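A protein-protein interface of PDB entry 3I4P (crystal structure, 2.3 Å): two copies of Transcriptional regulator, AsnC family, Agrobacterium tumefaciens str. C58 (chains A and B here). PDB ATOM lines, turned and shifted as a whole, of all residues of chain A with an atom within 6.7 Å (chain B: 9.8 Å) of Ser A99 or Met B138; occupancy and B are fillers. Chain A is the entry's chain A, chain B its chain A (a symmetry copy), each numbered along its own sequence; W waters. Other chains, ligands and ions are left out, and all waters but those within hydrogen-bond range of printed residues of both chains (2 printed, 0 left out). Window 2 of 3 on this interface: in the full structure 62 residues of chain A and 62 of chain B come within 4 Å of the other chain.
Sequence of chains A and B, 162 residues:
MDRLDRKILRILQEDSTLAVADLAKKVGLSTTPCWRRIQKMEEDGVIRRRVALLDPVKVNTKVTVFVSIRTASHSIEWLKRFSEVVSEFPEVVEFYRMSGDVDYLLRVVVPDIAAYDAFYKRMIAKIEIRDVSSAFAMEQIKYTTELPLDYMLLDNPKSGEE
Of the printed residues of chain B, Arg A97 touches Ala B137 (3.7 Å), Met B138 (2.8 Å), Glu B139 (3.0 Å) and Ile B141 (3.9 Å).
Ser A99 touches just these residues of chain B: Phe B136 and Met B138.
No residue of chain B comes within 4 Å of Gly A100.
Of the printed residues of chain A, Thr B64 touches Tyr A96.
Ser B133 touches none of the printed residues of chain A.
Printed residues of chain A within 4 Å of Ala B135: Met A98.
Met B138 touches three residues of chain A.
No position is printed for both chains.
Of the 16 pairs that touch across the chains among the printed residues, none has its exchanged pair printed and touching as well.
NE2 of Gln B140 sits at hydrogen-bond distance from OH of Tyr A96 (3.2 Å).
O of Arg A97 sits at hydrogen-bond distance from N of Met B138, 2.8 Å away.
The side-chain carboxylate of Glu B139 is in salt-bridge range of the guanidinium group of Arg A97 (3.3 Å).
OG of Ser A99 lies within hydrogen-bond range of O of Phe B136 (2.8 Å).
The backbone NH of Met A98 lies within hydrogen-bond range of the backbone carbonyl oxygen of Asp A103 (2.8 Å).
N of Ala B137 lies within hydrogen-bond range of O of Thr B64 (2.9 Å).
N of Phe B66 is in hydrogen-bond range of O of Ala B135.
Among the printed residues, pairs that only touch across the chains: Met A98 with Ala B135 (3.3 Å), Tyr A96 with Glu B139 (3.4 Å), Ser A99 with Met B138 (3.6 Å), Tyr A96 with Phe B66 (3.7 Å), Arg A97 with Ala B137 (3.7 Å), Met A98 with Phe B66 (3.8 Å), Tyr A96 with Ala B137 (3.8 Å), Tyr A96 with Thr B64 (3.8 Å), Met A98 with Ala B137 (3.9 Å), Met A98 with Phe B136 (3.9 Å), Arg A97 with Ile B141 (3.9 Å) and Met A98 with Met B138 (3.9 Å).
Water W2 lies within hydrogen-bond range of OG of Ser A99 (2.6 Å) and N of Phe B136 (3.1 Å).
Water W1 bridges OE1 of Glu B139 (3.4 Å) and NH2 of Arg A97 (3.5 Å).
Of the 15 printed residues of chain B, 9 touch a printed residue of chain A.
Hydrophobic or aromatic side chains of chain B within 4 Å of the printed part of chain A: Phe B66, Ala B135, Ala B137, Met B138 and Ile B141.
Hydrophobic or aromatic side chains of chain A that line the printed part of chain B: Tyr A96 and Met A98.
Among the printed residues, Asp or Glu carboxylates within 4 Å of a Lys or Arg side-chain nitrogen of the other chain: Arg A97 with Glu B139 (3.3 Å).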
ATOM      1  N   TYR A  96      -4.362   3.325  20.613  1.00  0.00           N
ATOM      2  CA  TYR A  96      -4.884   4.561  21.173  1.00  0.00           C
ATOM      3  C   TYR A  96      -4.455   5.747  20.382  1.00  0.00           C
ATOM      4  O   TYR A  96      -3.289   5.859  19.959  1.00  0.00           O
ATOM      5  CB  TYR A  96      -4.388   4.805  22.622  1.00  0.00           C
ATOM      6  CG  TYR A  96      -4.825   3.750  23.577  1.00  0.00           C
ATOM      7  CD1 TYR A  96      -6.000   3.871  24.300  1.00  0.00           C
ATOM      8  CD2 TYR A  96      -4.086   2.594  23.718  1.00  0.00           C
ATOM      9  CE1 TYR A  96      -6.392   2.881  25.149  1.00  0.00           C
ATOM     10  CE2 TYR A  96      -4.489   1.591  24.535  1.00  0.00           C
ATOM     11  CZ  TYR A  96      -5.631   1.731  25.249  1.00  0.00           C
ATOM     12  OH  TYR A  96      -5.998   0.695  26.073  1.00  0.00           O
ATOM     13  N   ARG A  97      -5.398   6.665  20.240  1.00  0.00           N
ATOM     14  CA  ARG A  97      -5.119   7.980  19.743  1.00  0.00           C
ATOM     15  C   ARG A  97      -4.745   8.776  20.975  1.00  0.00           C
ATOM     16  O   ARG A  97      -5.517   8.836  21.921  1.00  0.00           O
ATOM     17  CB  ARG A  97      -6.333   8.563  19.014  1.00  0.00           C
ATOM     18  CG  ARG A  97      -6.099   9.961  18.517  1.00  0.00           C
ATOM     19  CD  ARG A  97      -7.095  10.359  17.406  1.00  0.00           C
ATOM     20  NE  ARG A  97      -8.458  10.284  17.922  1.00  0.00           N
ATOM     21  CZ  ARG A  97      -9.059  11.235  18.624  1.00  0.00           C
ATOM     22  NH1 ARG A  97      -8.434  12.377  18.894  1.00  0.00           N
ATOM     23  NH2 ARG A  97     -10.304  11.043  19.053  1.00  0.00           N
ATOM     24  N   MET A  98      -3.530   9.324  20.985  1.00  0.00           N
ATOM     25  CA  MET A  98      -2.998   9.981  22.150  1.00  0.00           C
ATOM     26  C   MET A  98      -3.013  11.493  21.994  1.00  0.00           C
ATOM     27  O   MET A  98      -3.161  12.040  20.879  1.00  0.00           O
ATOM     28  CB  MET A  98      -1.560   9.556  22.400  1.00  0.00           C
ATOM     29  CG  MET A  98      -1.334   8.067  22.634  1.00  0.00           C
ATOM     30  SD  MET A  98      -2.102   7.404  24.255  1.00  0.00           S
ATOM     31  CE  MET A  98      -1.215   8.320  25.646  1.00  0.00           C
ATOM     32  N   SER A  99      -2.870  12.141  23.148  1.00  0.00           N
ATOM     33  CA  SER A  99      -2.561  13.544  23.249  1.00  0.00           C
ATOM     34  C   SER A  99      -1.098  13.544  23.660  1.00  0.00           C
ATOM     35  O   SER A  99      -0.578  12.510  24.059  1.00  0.00           O
ATOM     36  CB  SER A  99      -3.433  14.208  24.327  1.00  0.00           C
ATOM     37  OG  SER A  99      -2.979  13.850  25.637  1.00  0.00           O
ATOM     38  N   GLY A 100      -0.432  14.691  23.548  1.00  0.00           N
ATOM     39  CA  GLY A 100       0.975  14.811  23.952  1.00  0.00           C
ATOM     40  C   GLY A 100       1.881  14.745  22.738  1.00  0.00           C
ATOM     41  O   GLY A 100       1.453  14.987  21.624  1.00  0.00           O
ATOM     42  N   ASP A 101       3.142  14.408  22.960  1.00  0.00           N
ATOM     43  CA  ASP A 101       4.134  14.367  21.889  1.00  0.00           C
ATOM     44  C   ASP A 101       3.834  13.350  20.785  1.00  0.00           C
ATOM     45  O   ASP A 101       4.220  13.537  19.640  1.00  0.00           O
ATOM     46  CB  ASP A 101       5.507  14.061  22.482  1.00  0.00           C
ATOM     47  CG  ASP A 101       6.186  15.285  23.048  1.00  0.00           C
ATOM     48  OD1 ASP A 101       5.555  16.378  23.166  1.00  0.00           O
ATOM     49  OD2 ASP A 101       7.395  15.154  23.343  1.00  0.00           O
ATOM     50  N   VAL A 102       3.151  12.268  21.146  1.00  0.00           N
ATOM     51  CA  VAL A 102       2.901  11.176  20.231  1.00  0.00           C
ATOM     52  C   VAL A 102       1.425  11.190  19.818  1.00  0.00           C
ATOM     53  O   VAL A 102       0.564  11.499  20.617  1.00  0.00           O
ATOM     54  CB  VAL A 102       3.348   9.853  20.891  1.00  0.00           C
ATOM     55  CG1 VAL A 102       2.602   8.681  20.352  1.00  0.00           C
ATOM     56  CG2 VAL A 102       4.868   9.693  20.727  1.00  0.00           C
ATOM     57  N   ASP A 103       1.163  10.859  18.556  1.00  0.00           N
ATOM     58  CA  ASP A 103      -0.177  10.866  17.976  1.00  0.00           C
ATOM     59  C   ASP A 103      -0.933   9.567  18.291  1.00  0.00           C
ATOM     60  O   ASP A 103      -2.137   9.608  18.568  1.00  0.00           O
ATOM     61  CB  ASP A 103      -0.099  10.988  16.429  1.00  0.00           C
ATOM     62  CG  ASP A 103       0.211  12.397  15.943  1.00  0.00           C
ATOM     63  OD1 ASP A 103      -0.366  13.361  16.498  1.00  0.00           O
ATOM     64  OD2 ASP A 103       0.978  12.539  14.961  1.00  0.00           O
ATOM     65  N   LYS B  62     -13.622   5.603  31.869  1.00  0.00           N
ATOM     66  CA  LYS B  62     -13.493   5.856  30.413  1.00  0.00           C
ATOM     67  C   LYS B  62     -12.193   6.508  29.970  1.00  0.00           C
ATOM     68  O   LYS B  62     -11.920   6.548  28.771  1.00  0.00           O
ATOM     69  CB  LYS B  62     -14.670   6.699  29.876  1.00  0.00           C
ATOM     70  CG  LYS B  62     -14.614   8.182  30.230  1.00  0.00           C
ATOM     71  CD  LYS B  62     -15.968   8.932  30.020  1.00  0.00           C
ATOM     72  CE  LYS B  62     -15.907  10.411  30.546  1.00  0.00           C
ATOM     73  NZ  LYS B  62     -15.830  10.609  32.080  1.00  0.00           N
ATOM     74  N   VAL B  63     -11.412   7.054  30.909  1.00  0.00           N
ATOM     75  CA  VAL B  63     -10.131   7.706  30.556  1.00  0.00           C
ATOM     76  C   VAL B  63      -8.993   6.704  30.787  1.00  0.00           C
ATOM     77  O   VAL B  63      -8.937   6.021  31.810  1.00  0.00           O
ATOM     78  CB  VAL B  63      -9.892   9.026  31.334  1.00  0.00           C
ATOM     79  CG1 VAL B  63      -8.445   9.555  31.087  1.00  0.00           C
ATOM     80  CG2 VAL B  63     -10.961  10.089  30.966  1.00  0.00           C
ATOM     81  N   THR B  64      -8.126   6.590  29.791  1.00  0.00           N
ATOM     82  CA  THR B  64      -6.868   5.864  29.884  1.00  0.00           C
ATOM     83  C   THR B  64      -5.703   6.867  29.948  1.00  0.00           C
ATOM     84  O   THR B  64      -5.614   7.798  29.165  1.00  0.00           O
ATOM     85  CB  THR B  64      -6.643   4.936  28.645  1.00  0.00           C
ATOM     86  OG1 THR B  64      -7.650   3.924  28.617  1.00  0.00           O
ATOM     87  CG2 THR B  64      -5.296   4.280  28.700  1.00  0.00           C
ATOM     88  N   VAL B  65      -4.803   6.632  30.890  1.00  0.00           N
ATOM     89  CA  VAL B  65      -3.605   7.413  31.068  1.00  0.00           C
ATOM     90  C   VAL B  65      -2.443   6.429  30.974  1.00  0.00           C
ATOM     91  O   VAL B  65      -2.463   5.380  31.607  1.00  0.00           O
ATOM     92  CB  VAL B  65      -3.593   8.042  32.468  1.00  0.00           C
ATOM     93  CG1 VAL B  65      -2.431   9.021  32.580  1.00  0.00           C
ATOM     94  CG2 VAL B  65      -4.944   8.666  32.757  1.00  0.00           C
ATOM     95  N   PHE B  66      -1.435   6.774  30.203  1.00  0.00           N
ATOM     96  CA  PHE B  66      -0.201   5.993  30.145  1.00  0.00           C
ATOM     97  C   PHE B  66       0.836   6.722  30.969  1.00  0.00           C
ATOM     98  O   PHE B  66       1.213   7.864  30.650  1.00  0.00           O
ATOM     99  CB  PHE B  66       0.281   5.793  28.694  1.00  0.00           C
ATOM    100  CG  PHE B  66      -0.423   4.677  28.009  1.00  0.00           C
ATOM    101  CD1 PHE B  66       0.008   3.374  28.175  1.00  0.00           C
ATOM    102  CD2 PHE B  66      -1.578   4.922  27.270  1.00  0.00           C
ATOM    103  CE1 PHE B  66      -0.675   2.308  27.553  1.00  0.00           C
ATOM    104  CE2 PHE B  66      -2.252   3.902  26.678  1.00  0.00           C
ATOM    105  CZ  PHE B  66      -1.796   2.581  26.810  1.00  0.00           C
ATOM    106  N   ILE B 113      -9.801  13.523  34.659  1.00  0.00           N
ATOM    107  CA  ILE B 113      -8.538  14.107  35.098  1.00  0.00           C
ATOM    108  C   ILE B 113      -8.458  14.208  36.632  1.00  0.00           C
ATOM    109  O   ILE B 113      -7.453  13.831  37.215  1.00  0.00           O
ATOM    110  CB  ILE B 113      -8.282  15.506  34.401  1.00  0.00           C
ATOM    111  CG1 ILE B 113      -7.809  15.304  32.970  1.00  0.00           C
ATOM    112  CG2 ILE B 113      -7.274  16.379  35.141  1.00  0.00           C
ATOM    113  CD1 ILE B 113      -7.924  16.612  32.108  1.00  0.00           C
ATOM    114  N   SER B 133       5.921  10.790  33.933  1.00  0.00           N
ATOM    115  CA  SER B 133       5.330  11.589  32.863  1.00  0.00           C
ATOM    116  C   SER B 133       4.074  10.865  32.469  1.00  0.00           C
ATOM    117  O   SER B 133       4.141   9.710  32.020  1.00  0.00           O
ATOM    118  CB  SER B 133       6.280  11.768  31.675  1.00  0.00           C
ATOM    119  OG  SER B 133       5.630  12.396  30.549  1.00  0.00           O
ATOM    120  N   SER B 134       2.929  11.508  32.695  1.00  0.00           N
ATOM    121  CA  SER B 134       1.639  10.958  32.318  1.00  0.00           C
ATOM    122  C   SER B 134       1.184  11.481  30.945  1.00  0.00           C
ATOM    123  O   SER B 134       1.345  12.655  30.634  1.00  0.00           O
ATOM    124  CB  SER B 134       0.592  11.272  33.387  1.00  0.00           C
ATOM    125  OG  SER B 134       1.051  10.921  34.704  1.00  0.00           O
ATOM    126  N   ALA B 135       0.612  10.599  30.135  1.00  0.00           N
ATOM    127  CA  ALA B 135       0.021  10.944  28.824  1.00  0.00           C
ATOM    128  C   ALA B 135      -1.408  10.344  28.747  1.00  0.00           C
ATOM    129  O   ALA B 135      -1.593   9.123  28.866  1.00  0.00           O
ATOM    130  CB  ALA B 135       0.875  10.394  27.683  1.00  0.00           C
ATOM    131  N   PHE B 136      -2.386  11.205  28.502  1.00  0.00           N
ATOM    132  CA  PHE B 136      -3.795  10.832  28.399  1.00  0.00           C
ATOM    133  C   PHE B 136      -4.168  10.448  26.985  1.00  0.00           C
ATOM    134  O   PHE B 136      -3.896  11.195  26.036  1.00  0.00           O
ATOM    135  CB  PHE B 136      -4.700  12.016  28.826  1.00  0.00           C
ATOM    136  CG  PHE B 136      -4.568  12.375  30.295  1.00  0.00           C
ATOM    137  CD1 PHE B 136      -5.467  11.895  31.225  1.00  0.00           C
ATOM    138  CD2 PHE B 136      -3.528  13.199  30.733  1.00  0.00           C
ATOM    139  CE1 PHE B 136      -5.331  12.231  32.585  1.00  0.00           C
ATOM    140  CE2 PHE B 136      -3.379  13.527  32.070  1.00  0.00           C
ATOM    141  CZ  PHE B 136      -4.279  13.027  33.006  1.00  0.00           C
ATOM    142  N   ALA B 137      -4.800   9.283  26.863  1.00  0.00           N
ATOM    143  CA  ALA B 137      -5.421   8.837  25.629  1.00  0.00           C
ATOM    144  C   ALA B 137      -6.636   9.730  25.296  1.00  0.00           C
ATOM    145  O   ALA B 137      -7.433  10.044  26.177  1.00  0.00           O
ATOM    146  CB  ALA B 137      -5.851   7.367  25.766  1.00  0.00           C
ATOM    147  N   MET B 138      -6.767  10.118  24.019  1.00  0.00           N
ATOM    148  CA  MET B 138      -7.963  10.783  23.483  1.00  0.00           C
ATOM    149  C   MET B 138      -9.033   9.795  23.063  1.00  0.00           C
ATOM    150  O   MET B 138     -10.204  10.131  23.107  1.00  0.00           O
ATOM    151  CB  MET B 138      -7.617  11.624  22.261  1.00  0.00           C
ATOM    152  CG  MET B 138      -6.693  12.804  22.560  1.00  0.00           C
ATOM    153  SD  MET B 138      -7.549  14.019  23.796  1.00  0.00           S
ATOM    154  CE  MET B 138      -6.786  13.278  25.406  1.00  0.00           C
ATOM    155  N   GLU B 139      -8.634   8.601  22.622  1.00  0.00           N
ATOM    156  CA  GLU B 139      -9.577   7.595  22.180  1.00  0.00           C
ATOM    157  C   GLU B 139      -8.938   6.223  22.289  1.00  0.00           C
ATOM    158  O   GLU B 139      -7.770   6.069  21.996  1.00  0.00           O
ATOM    159  CB  GLU B 139     -10.026   7.857  20.721  1.00  0.00           C
ATOM    160  CG  GLU B 139     -11.049   6.826  20.200  1.00  0.00           C
ATOM    161  CD  GLU B 139     -11.489   7.066  18.746  1.00  0.00           C
ATOM    162  OE1 GLU B 139     -10.977   8.010  18.083  1.00  0.00           O
ATOM    163  OE2 GLU B 139     -12.342   6.279  18.258  1.00  0.00           O
ATOM    164  N   GLN B 140      -9.719   5.236  22.718  1.00  0.00           N
ATOM    165  CA  GLN B 140      -9.365   3.830  22.564  1.00  0.00           C
ATOM    166  C   GLN B 140      -9.941   3.289  21.250  1.00  0.00           C
ATOM    167  O   GLN B 140     -11.133   2.976  21.165  1.00  0.00           O
ATOM    168  CB  GLN B 140      -9.886   3.040  23.744  1.00  0.00           C
ATOM    169  CG  GLN B 140      -9.410   1.615  23.860  1.00  0.00           C
ATOM    170  CD  GLN B 140     -10.047   0.951  25.099  1.00  0.00           C
ATOM    171  OE1 GLN B 140     -11.260   0.682  25.110  1.00  0.00           O
ATOM    172  NE2 GLN B 140      -9.228   0.700  26.146  1.00  0.00           N
ATOM    173  N   ILE B 141      -9.092   3.209  20.218  1.00  0.00           N
ATOM    174  CA  ILE B 141      -9.516   2.749  18.884  1.00  0.00           C
ATOM    175  C   ILE B 141      -9.698   1.245  18.862  1.00  0.00           C
ATOM    176  O   ILE B 141     -10.692   0.764  18.360  1.00  0.00           O
ATOM    177  CB  ILE B 141      -8.520   3.135  17.769  1.00  0.00           C
ATOM    178  CG1 ILE B 141      -8.404   4.662  17.667  1.00  0.00           C
ATOM    179  CG2 ILE B 141      -9.002   2.524  16.417  1.00  0.00           C
ATOM    180  CD1 ILE B 141      -7.128   5.143  17.051  1.00  0.00           C
HETATM  181  O   HOH W   1     -13.396   9.662  19.725  1.00  0.00           O
HETATM  182  O   HOH W   2      -1.447  14.082  27.719  1.00  0.00           O
